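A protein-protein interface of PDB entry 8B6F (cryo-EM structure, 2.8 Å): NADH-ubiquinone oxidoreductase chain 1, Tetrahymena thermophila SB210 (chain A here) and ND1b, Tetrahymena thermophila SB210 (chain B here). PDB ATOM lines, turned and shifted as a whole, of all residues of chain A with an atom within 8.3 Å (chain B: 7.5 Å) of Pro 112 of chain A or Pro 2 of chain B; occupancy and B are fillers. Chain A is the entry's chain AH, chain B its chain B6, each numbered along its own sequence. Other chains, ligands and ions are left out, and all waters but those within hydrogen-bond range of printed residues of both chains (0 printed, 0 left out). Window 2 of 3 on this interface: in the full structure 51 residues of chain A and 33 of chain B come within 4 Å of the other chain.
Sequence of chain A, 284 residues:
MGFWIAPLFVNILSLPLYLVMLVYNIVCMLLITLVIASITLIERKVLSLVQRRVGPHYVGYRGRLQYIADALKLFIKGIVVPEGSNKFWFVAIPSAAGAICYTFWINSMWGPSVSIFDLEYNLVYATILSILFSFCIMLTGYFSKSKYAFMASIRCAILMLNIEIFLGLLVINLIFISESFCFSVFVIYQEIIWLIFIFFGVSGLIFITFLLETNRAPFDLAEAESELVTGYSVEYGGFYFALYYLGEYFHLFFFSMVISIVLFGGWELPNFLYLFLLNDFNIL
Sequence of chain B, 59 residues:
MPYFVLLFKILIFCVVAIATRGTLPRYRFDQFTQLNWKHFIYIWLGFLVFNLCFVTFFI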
ATOM      1  N   MET A 109     -28.436 -13.268  27.621  1.00  0.00           N
ATOM      2  CA  MET A 109     -27.456 -13.271  26.545  1.00  0.00           C
ATOM      3  C   MET A 109     -27.465 -14.624  25.850  1.00  0.00           C
ATOM      4  O   MET A 109     -27.570 -15.668  26.502  1.00  0.00           O
ATOM      5  CB  MET A 109     -26.050 -12.966  27.058  1.00  0.00           C
ATOM      6  CG  MET A 109     -25.900 -11.555  27.601  1.00  0.00           C
ATOM      7  SD  MET A 109     -24.209 -10.936  27.522  1.00  0.00           S
ATOM      8  CE  MET A 109     -23.965 -10.869  25.748  1.00  0.00           C
ATOM      9  N   TRP A 110     -27.354 -14.596  24.523  1.00  0.00           N
ATOM     10  CA  TRP A 110     -27.404 -15.800  23.702  1.00  0.00           C
ATOM     11  C   TRP A 110     -26.180 -15.895  22.800  1.00  0.00           C
ATOM     12  O   TRP A 110     -26.250 -16.447  21.700  1.00  0.00           O
ATOM     13  CB  TRP A 110     -28.686 -15.826  22.870  1.00  0.00           C
ATOM     14  CG  TRP A 110     -29.919 -15.648  23.694  1.00  0.00           C
ATOM     15  CD1 TRP A 110     -30.645 -14.504  23.845  1.00  0.00           C
ATOM     16  CD2 TRP A 110     -30.568 -16.645  24.490  1.00  0.00           C
ATOM     17  NE1 TRP A 110     -31.708 -14.727  24.685  1.00  0.00           N
ATOM     18  CE2 TRP A 110     -31.682 -16.034  25.094  1.00  0.00           C
ATOM     19  CE3 TRP A 110     -30.313 -17.995  24.749  1.00  0.00           C
ATOM     20  CZ2 TRP A 110     -32.543 -16.726  25.942  1.00  0.00           C
ATOM     21  CZ3 TRP A 110     -31.167 -18.681  25.590  1.00  0.00           C
ATOM     22  CH2 TRP A 110     -32.270 -18.046  26.178  1.00  0.00           C
ATOM     23  N   GLY A 111     -25.051 -15.366  23.259  1.00  0.00           N
ATOM     24  CA  GLY A 111     -23.837 -15.345  22.480  1.00  0.00           C
ATOM     25  C   GLY A 111     -22.851 -14.350  23.052  1.00  0.00           C
ATOM     26  O   GLY A 111     -23.091 -13.744  24.100  1.00  0.00           O
ATOM     27  N   PRO A 112     -21.720 -14.155  22.371  1.00  0.00           N
ATOM     28  CA  PRO A 112     -20.723 -13.209  22.897  1.00  0.00           C
ATOM     29  C   PRO A 112     -21.285 -11.820  23.143  1.00  0.00           C
ATOM     30  O   PRO A 112     -20.957 -11.195  24.158  1.00  0.00           O
ATOM     31  CB  PRO A 112     -19.641 -13.208  21.808  1.00  0.00           C
ATOM     32  CG  PRO A 112     -19.792 -14.517  21.121  1.00  0.00           C
ATOM     33  CD  PRO A 112     -21.255 -14.830  21.150  1.00  0.00           C
ATOM     34  N   SER A 113     -22.124 -11.313  22.236  1.00  0.00           N
ATOM     35  CA  SER A 113     -22.790 -10.032  22.436  1.00  0.00           C
ATOM     36  C   SER A 113     -24.228 -10.073  21.940  1.00  0.00           C
ATOM     37  O   SER A 113     -24.792  -9.038  21.568  1.00  0.00           O
ATOM     38  CB  SER A 113     -22.023  -8.906  21.750  1.00  0.00           C
ATOM     39  OG  SER A 113     -20.742  -8.773  22.338  1.00  0.00           O
ATOM     40  N   VAL A 114     -24.836 -11.255  21.929  1.00  0.00           N
ATOM     41  CA  VAL A 114     -26.189 -11.421  21.376  1.00  0.00           C
ATOM     42  C   VAL A 114     -27.149 -11.147  22.527  1.00  0.00           C
ATOM     43  O   VAL A 114     -27.623 -12.043  23.229  1.00  0.00           O
ATOM     44  CB  VAL A 114     -26.389 -12.804  20.751  1.00  0.00           C
ATOM     45  CG1 VAL A 114     -27.745 -12.890  20.072  1.00  0.00           C
ATOM     46  CG2 VAL A 114     -25.271 -13.111  19.766  1.00  0.00           C
ATOM     47  N   SER A 115     -27.444  -9.865  22.724  1.00  0.00           N
ATOM     48  CA  SER A 115     -28.396  -9.425  23.731  1.00  0.00           C
ATOM     49  C   SER A 115     -29.234  -8.301  23.145  1.00  0.00           C
ATOM     50  O   SER A 115     -28.748  -7.500  22.344  1.00  0.00           O
ATOM     51  CB  SER A 115     -27.685  -8.946  25.001  1.00  0.00           C
ATOM     52  OG  SER A 115     -28.614  -8.575  26.002  1.00  0.00           O
ATOM     53  N   CYS A 182     -21.061  -8.780  33.511  1.00  0.00           N
ATOM     54  CA  CYS A 182     -21.590  -9.237  32.235  1.00  0.00           C
ATOM     55  C   CYS A 182     -21.416 -10.743  32.090  1.00  0.00           C
ATOM     56  O   CYS A 182     -20.391 -11.306  32.480  1.00  0.00           O
ATOM     57  CB  CYS A 182     -20.891  -8.519  31.081  1.00  0.00           C
ATOM     58  SG  CYS A 182     -21.559  -8.910  29.449  1.00  0.00           S
ATOM     59  N   PHE A 183     -22.430 -11.392  31.518  1.00  0.00           N
ATOM     60  CA  PHE A 183     -22.380 -12.839  31.345  1.00  0.00           C
ATOM     61  C   PHE A 183     -21.313 -13.265  30.343  1.00  0.00           C
ATOM     62  O   PHE A 183     -20.774 -14.371  30.451  1.00  0.00           O
ATOM     63  CB  PHE A 183     -23.746 -13.359  30.896  1.00  0.00           C
ATOM     64  CG  PHE A 183     -24.839 -13.170  31.908  1.00  0.00           C
ATOM     65  CD1 PHE A 183     -24.576 -13.255  33.266  1.00  0.00           C
ATOM     66  CD2 PHE A 183     -26.137 -12.924  31.496  1.00  0.00           C
ATOM     67  CE1 PHE A 183     -25.585 -13.087  34.191  1.00  0.00           C
ATOM     68  CE2 PHE A 183     -27.150 -12.757  32.417  1.00  0.00           C
ATOM     69  CZ  PHE A 183     -26.874 -12.840  33.767  1.00  0.00           C
ATOM     70  N   SER A 184     -20.999 -12.415  29.364  1.00  0.00           N
ATOM     71  CA  SER A 184     -20.066 -12.815  28.315  1.00  0.00           C
ATOM     72  C   SER A 184     -18.681 -13.105  28.875  1.00  0.00           C
ATOM     73  O   SER A 184     -18.013 -14.050  28.444  1.00  0.00           O
ATOM     74  CB  SER A 184     -19.983 -11.724  27.250  1.00  0.00           C
ATOM     75  OG  SER A 184     -21.249 -11.479  26.673  1.00  0.00           O
ATOM     76  N   VAL A 185     -18.231 -12.299  29.838  1.00  0.00           N
ATOM     77  CA  VAL A 185     -16.862 -12.400  30.328  1.00  0.00           C
ATOM     78  C   VAL A 185     -16.588 -13.742  30.992  1.00  0.00           C
ATOM     79  O   VAL A 185     -15.424 -14.118  31.161  1.00  0.00           O
ATOM     80  CB  VAL A 185     -16.556 -11.210  31.257  1.00  0.00           C
ATOM     81  CG1 VAL A 185     -15.120 -11.253  31.748  1.00  0.00           C
ATOM     82  CG2 VAL A 185     -16.801  -9.915  30.490  1.00  0.00           C
ATOM     83  N   VAL A 187     -17.596 -16.786  29.794  1.00  0.00           N
ATOM     84  CA  VAL A 187     -17.376 -17.843  28.813  1.00  0.00           C
ATOM     85  C   VAL A 187     -15.936 -17.829  28.312  1.00  0.00           C
ATOM     86  O   VAL A 187     -15.350 -18.884  28.047  1.00  0.00           O
ATOM     87  CB  VAL A 187     -18.382 -17.715  27.656  1.00  0.00           C
ATOM     88  CG1 VAL A 187     -18.093 -18.751  26.582  1.00  0.00           C
ATOM     89  CG2 VAL A 187     -19.796 -17.876  28.183  1.00  0.00           C
ATOM     90  N   ILE A 188     -15.344 -16.643  28.165  1.00  0.00           N
ATOM     91  CA  ILE A 188     -13.972 -16.561  27.664  1.00  0.00           C
ATOM     92  C   ILE A 188     -13.019 -17.294  28.599  1.00  0.00           C
ATOM     93  O   ILE A 188     -12.062 -17.936  28.151  1.00  0.00           O
ATOM     94  CB  ILE A 188     -13.553 -15.093  27.461  1.00  0.00           C
ATOM     95  CG1 ILE A 188     -13.699 -14.296  28.760  1.00  0.00           C
ATOM     96  CG2 ILE A 188     -14.384 -14.466  26.352  1.00  0.00           C
ATOM     97  CD1 ILE A 188     -13.127 -12.896  28.692  1.00  0.00           C
ATOM     98  N   GLU A 191     -13.703 -21.317  28.436  1.00  0.00           N
ATOM     99  CA  GLU A 191     -13.439 -22.043  27.197  1.00  0.00           C
ATOM    100  C   GLU A 191     -12.652 -23.322  27.461  1.00  0.00           C
ATOM    101  O   GLU A 191     -13.012 -24.397  26.970  1.00  0.00           O
ATOM    102  CB  GLU A 191     -12.689 -21.147  26.210  1.00  0.00           C
ATOM    103  CG  GLU A 191     -13.508 -19.971  25.694  1.00  0.00           C
ATOM    104  CD  GLU A 191     -12.829 -19.243  24.548  1.00  0.00           C
ATOM    105  OE1 GLU A 191     -11.716 -19.652  24.160  1.00  0.00           O
ATOM    106  OE2 GLU A 191     -13.411 -18.263  24.036  1.00  0.00           O
ATOM    107  N   GLY A 265     -19.765 -23.109  31.371  1.00  0.00           N
ATOM    108  CA  GLY A 265     -19.242 -22.768  30.067  1.00  0.00           C
ATOM    109  C   GLY A 265     -20.203 -22.047  29.153  1.00  0.00           C
ATOM    110  O   GLY A 265     -19.789 -21.606  28.074  1.00  0.00           O
ATOM    111  N   GLY A 266     -21.466 -21.901  29.540  1.00  0.00           N
ATOM    112  CA  GLY A 266     -22.426 -21.235  28.689  1.00  0.00           C
ATOM    113  C   GLY A 266     -22.557 -21.903  27.338  1.00  0.00           C
ATOM    114  O   GLY A 266     -23.107 -23.002  27.228  1.00  0.00           O
ATOM    115  N   TRP A 267     -22.046 -21.245  26.300  1.00  0.00           N
ATOM    116  CA  TRP A 267     -22.147 -21.731  24.929  1.00  0.00           C
ATOM    117  C   TRP A 267     -20.853 -22.378  24.447  1.00  0.00           C
ATOM    118  O   TRP A 267     -20.578 -22.392  23.242  1.00  0.00           O
ATOM    119  CB  TRP A 267     -22.556 -20.591  23.997  1.00  0.00           C
ATOM    120  CG  TRP A 267     -21.759 -19.333  24.179  1.00  0.00           C
ATOM    121  CD1 TRP A 267     -20.553 -19.040  23.618  1.00  0.00           C
ATOM    122  CD2 TRP A 267     -22.117 -18.200  24.978  1.00  0.00           C
ATOM    123  NE1 TRP A 267     -20.136 -17.794  24.018  1.00  0.00           N
ATOM    124  CE2 TRP A 267     -21.078 -17.258  24.855  1.00  0.00           C
ATOM    125  CE3 TRP A 267     -23.215 -17.891  25.788  1.00  0.00           C
ATOM    126  CZ2 TRP A 267     -21.104 -16.027  25.507  1.00  0.00           C
ATOM    127  CZ3 TRP A 267     -23.240 -16.670  26.436  1.00  0.00           C
ATOM    128  CH2 TRP A 267     -22.190 -15.753  26.293  1.00  0.00           C
ATOM    129  N   GLU A 268     -20.055 -22.915  25.363  1.00  0.00           N
ATOM    130  CA  GLU A 268     -18.832 -23.631  25.028  1.00  0.00           C
ATOM    131  C   GLU A 268     -19.036 -25.119  25.270  1.00  0.00           C
ATOM    132  O   GLU A 268     -19.519 -25.518  26.335  1.00  0.00           O
ATOM    133  CB  GLU A 268     -17.653 -23.116  25.857  1.00  0.00           C
ATOM    134  CG  GLU A 268     -17.106 -21.778  25.389  1.00  0.00           C
ATOM    135  CD  GLU A 268     -16.430 -21.862  24.031  1.00  0.00           C
ATOM    136  OE1 GLU A 268     -16.245 -22.988  23.525  1.00  0.00           O
ATOM    137  OE2 GLU A 268     -16.087 -20.802  23.469  1.00  0.00           O
ATOM    138  N   LEU A 269     -18.664 -25.931  24.285  1.00  0.00           N
ATOM    139  CA  LEU A 269     -18.806 -27.371  24.402  1.00  0.00           C
ATOM    140  C   LEU A 269     -17.861 -27.908  25.471  1.00  0.00           C
ATOM    141  O   LEU A 269     -16.848 -27.283  25.792  1.00  0.00           O
ATOM    142  CB  LEU A 269     -18.521 -28.044  23.062  1.00  0.00           C
ATOM    143  CG  LEU A 269     -19.607 -27.907  21.992  1.00  0.00           C
ATOM    144  CD1 LEU A 269     -19.103 -28.423  20.657  1.00  0.00           C
ATOM    145  CD2 LEU A 269     -20.868 -28.649  22.402  1.00  0.00           C
ATOM    146  N   MET B   1     -24.441 -21.919  15.967  1.00  0.00           N
ATOM    147  CA  MET B   1     -24.356 -20.695  16.813  1.00  0.00           C
ATOM    148  C   MET B   1     -24.319 -21.058  18.291  1.00  0.00           C
ATOM    149  O   MET B   1     -24.782 -22.129  18.683  1.00  0.00           O
ATOM    150  CB  MET B   1     -25.537 -19.765  16.530  1.00  0.00           C
ATOM    151  CG  MET B   1     -25.382 -18.947  15.262  1.00  0.00           C
ATOM    152  SD  MET B   1     -24.047 -17.742  15.373  1.00  0.00           S
ATOM    153  CE  MET B   1     -24.076 -17.054  13.722  1.00  0.00           C
ATOM    154  N   PRO B   2     -23.770 -20.164  19.114  1.00  0.00           N
ATOM    155  CA  PRO B   2     -23.642 -20.480  20.545  1.00  0.00           C
ATOM    156  C   PRO B   2     -24.962 -20.771  21.232  1.00  0.00           C
ATOM    157  O   PRO B   2     -24.996 -21.592  22.156  1.00  0.00           O
ATOM    158  CB  PRO B   2     -22.969 -19.224  21.121  1.00  0.00           C
ATOM    159  CG  PRO B   2     -23.201 -18.156  20.116  1.00  0.00           C
ATOM    160  CD  PRO B   2     -23.221 -18.837  18.793  1.00  0.00           C
ATOM    161  N   TYR B   3     -26.054 -20.128  20.819  1.00  0.00           N
ATOM    162  CA  TYR B   3     -27.316 -20.309  21.527  1.00  0.00           C
ATOM    163  C   TYR B   3     -27.863 -21.723  21.382  1.00  0.00           C
ATOM    164  O   TYR B   3     -28.663 -22.149  22.219  1.00  0.00           O
ATOM    165  CB  TYR B   3     -28.347 -19.280  21.058  1.00  0.00           C
ATOM    166  CG  TYR B   3     -28.608 -19.247  19.572  1.00  0.00           C
ATOM    167  CD1 TYR B   3     -29.428 -20.187  18.968  1.00  0.00           C
ATOM    168  CD2 TYR B   3     -28.061 -18.250  18.778  1.00  0.00           C
ATOM    169  CE1 TYR B   3     -29.680 -20.148  17.613  1.00  0.00           C
ATOM    170  CE2 TYR B   3     -28.305 -18.201  17.423  1.00  0.00           C
ATOM    171  CZ  TYR B   3     -29.116 -19.154  16.845  1.00  0.00           C
ATOM    172  OH  TYR B   3     -29.366 -19.111  15.495  1.00  0.00           O
ATOM    173  N   PHE B   4     -27.422 -22.478  20.375  1.00  0.00           N
ATOM    174  CA  PHE B   4     -27.826 -23.876  20.277  1.00  0.00           C
ATOM    175  C   PHE B   4     -27.324 -24.668  21.478  1.00  0.00           C
ATOM    176  O   PHE B   4     -28.100 -25.352  22.154  1.00  0.00           O
ATOM    177  CB  PHE B   4     -27.304 -24.476  18.971  1.00  0.00           C
ATOM    178  CG  PHE B   4     -27.916 -25.801  18.620  1.00  0.00           C
ATOM    179  CD1 PHE B   4     -29.268 -25.904  18.349  1.00  0.00           C
ATOM    180  CD2 PHE B   4     -27.133 -26.938  18.529  1.00  0.00           C
ATOM    181  CE1 PHE B   4     -29.834 -27.118  18.014  1.00  0.00           C
ATOM    182  CE2 PHE B   4     -27.693 -28.157  18.195  1.00  0.00           C
ATOM    183  CZ  PHE B   4     -29.046 -28.245  17.937  1.00  0.00           C
ATOM    184  N   VAL B   5     -26.025 -24.587  21.759  1.00  0.00           N
ATOM    185  CA  VAL B   5     -25.476 -25.276  22.922  1.00  0.00           C
ATOM    186  C   VAL B   5     -26.040 -24.688  24.210  1.00  0.00           C
ATOM    187  O   VAL B   5     -26.291 -25.411  25.180  1.00  0.00           O
ATOM    188  CB  VAL B   5     -23.939 -25.214  22.900  1.00  0.00           C
ATOM    189  CG1 VAL B   5     -23.358 -25.933  24.108  1.00  0.00           C
ATOM    190  CG2 VAL B   5     -23.405 -25.818  21.614  1.00  0.00           C
ATOM    191  N   LEU B   6     -26.245 -23.370  24.245  1.00  0.00           N
ATOM    192  CA  LEU B   6     -26.803 -22.743  25.440  1.00  0.00           C
ATOM    193  C   LEU B   6     -28.207 -23.259  25.725  1.00  0.00           C
ATOM    194  O   LEU B   6     -28.552 -23.533  26.879  1.00  0.00           O
ATOM    195  CB  LEU B   6     -26.804 -21.221  25.290  1.00  0.00           C
ATOM    196  CG  LEU B   6     -27.243 -20.418  26.520  1.00  0.00           C
ATOM    197  CD1 LEU B   6     -26.426 -20.782  27.754  1.00  0.00           C
ATOM    198  CD2 LEU B   6     -27.141 -18.929  26.243  1.00  0.00           C
ATOM    199  N   LEU B   7     -29.029 -23.411  24.685  1.00  0.00           N
ATOM    200  CA  LEU B   7     -30.365 -23.965  24.877  1.00  0.00           C
ATOM    201  C   LEU B   7     -30.299 -25.413  25.345  1.00  0.00           C
ATOM    202  O   LEU B   7     -31.097 -25.832  26.190  1.00  0.00           O
ATOM    203  CB  LEU B   7     -31.183 -23.851  23.588  1.00  0.00           C
ATOM    204  CG  LEU B   7     -32.062 -22.606  23.394  1.00  0.00           C
ATOM    205  CD1 LEU B   7     -33.147 -22.538  24.454  1.00  0.00           C
ATOM    206  CD2 LEU B   7     -31.264 -21.316  23.398  1.00  0.00           C
ATOM    207  N   PHE B   8     -29.364 -26.196  24.806  1.00  0.00           N
ATOM    208  CA  PHE B   8     -29.185 -27.561  25.290  1.00  0.00           C
ATOM    209  C   PHE B   8     -28.900 -27.575  26.786  1.00  0.00           C
ATOM    210  O   PHE B   8     -29.509 -28.342  27.539  1.00  0.00           O
ATOM    211  CB  PHE B   8     -28.050 -28.243  24.526  1.00  0.00           C
ATOM    212  CG  PHE B   8     -28.521 -29.182  23.459  1.00  0.00           C
ATOM    213  CD1 PHE B   8     -28.878 -30.482  23.771  1.00  0.00           C
ATOM    214  CD2 PHE B   8     -28.598 -28.768  22.140  1.00  0.00           C
ATOM    215  CE1 PHE B   8     -29.312 -31.350  22.789  1.00  0.00           C
ATOM    216  CE2 PHE B   8     -29.030 -29.631  21.152  1.00  0.00           C
ATOM    217  CZ  PHE B   8     -29.387 -30.924  21.477  1.00  0.00           C
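Leu 6 of chain B touches Met 109 of chain A. O of Trp 110 of chain A touches CG of Pro 2 of chain B (3.8 Å). CB of Tyr 3 of chain B touches O of Trp 110 of chain A, at 3.6 Å. CD2 of Leu 6 of chain B touches CE3 of Trp 110 of chain A (3.6 Å). Trp 110 of chain A touches Leu 7 of chain B (CZ3 to CD2, 3.4 Å). Pro 2 of chain B touches Gly 111 of chain A. Pro 112 of chain A touches Pro 2 of chain B (CD to CG, 3.99 Å). Trp 267 of chain A touches Pro 2 of chain B. Val 5 of chain B touches Leu 269 of chain A (CG2 to CD2, 3.9 Å).
Of the printed residues of chain B, Pro 112 of chain A touches Pro 2. Of the printed residues of chain A, Pro 2 of chain B touches Trp 110 (3.8 Å), Gly 111 (3.7 Å), Pro 112 (3.99 Å) and Trp 267 (3.2 Å). Of the printed residues of chain B, Leu 269 of chain A touches Val 5. Of the printed residues of chain B, Gly 111 of chain A touches Pro 2. Of the printed residues of chain B, Trp 267 of chain A touches Pro 2 (3.2 Å). Of the printed residues of chain A, Val 5 of chain B touches Leu 269. Phe 8 of chain B touches none of the printed residues of chain A. The nearest printed residue of chain B that does not touch Trp 110 of chain A is Met 1 of chain B (6.1 Å).
The backbone carbonyl oxygen (O) of Pro 112 of chain A sits at hydrogen-bond distance from the side-chain hydroxyl (OG) of Ser 184 of chain A. The side-chain sulfur (SD) of Met 109 of chain A sits close to the side-chain hydroxyl (OG) of Ser 184 of chain A, at 3.1 Å.
Printed residues of chain A that touch a printed residue of chain B: Met 109, Trp 110, Gly 111, Pro 112, Trp 267 and Leu 269. Hydrophobic or aromatic side chains of chain B that line the printed part of chain A: Pro 2, Tyr 3, Val 5, Leu 6 and Leu 7. Among the printed residues, no Asp or Glu carboxylate lies within 4 Å of a Lys or Arg side-chain nitrogen of the other chain.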
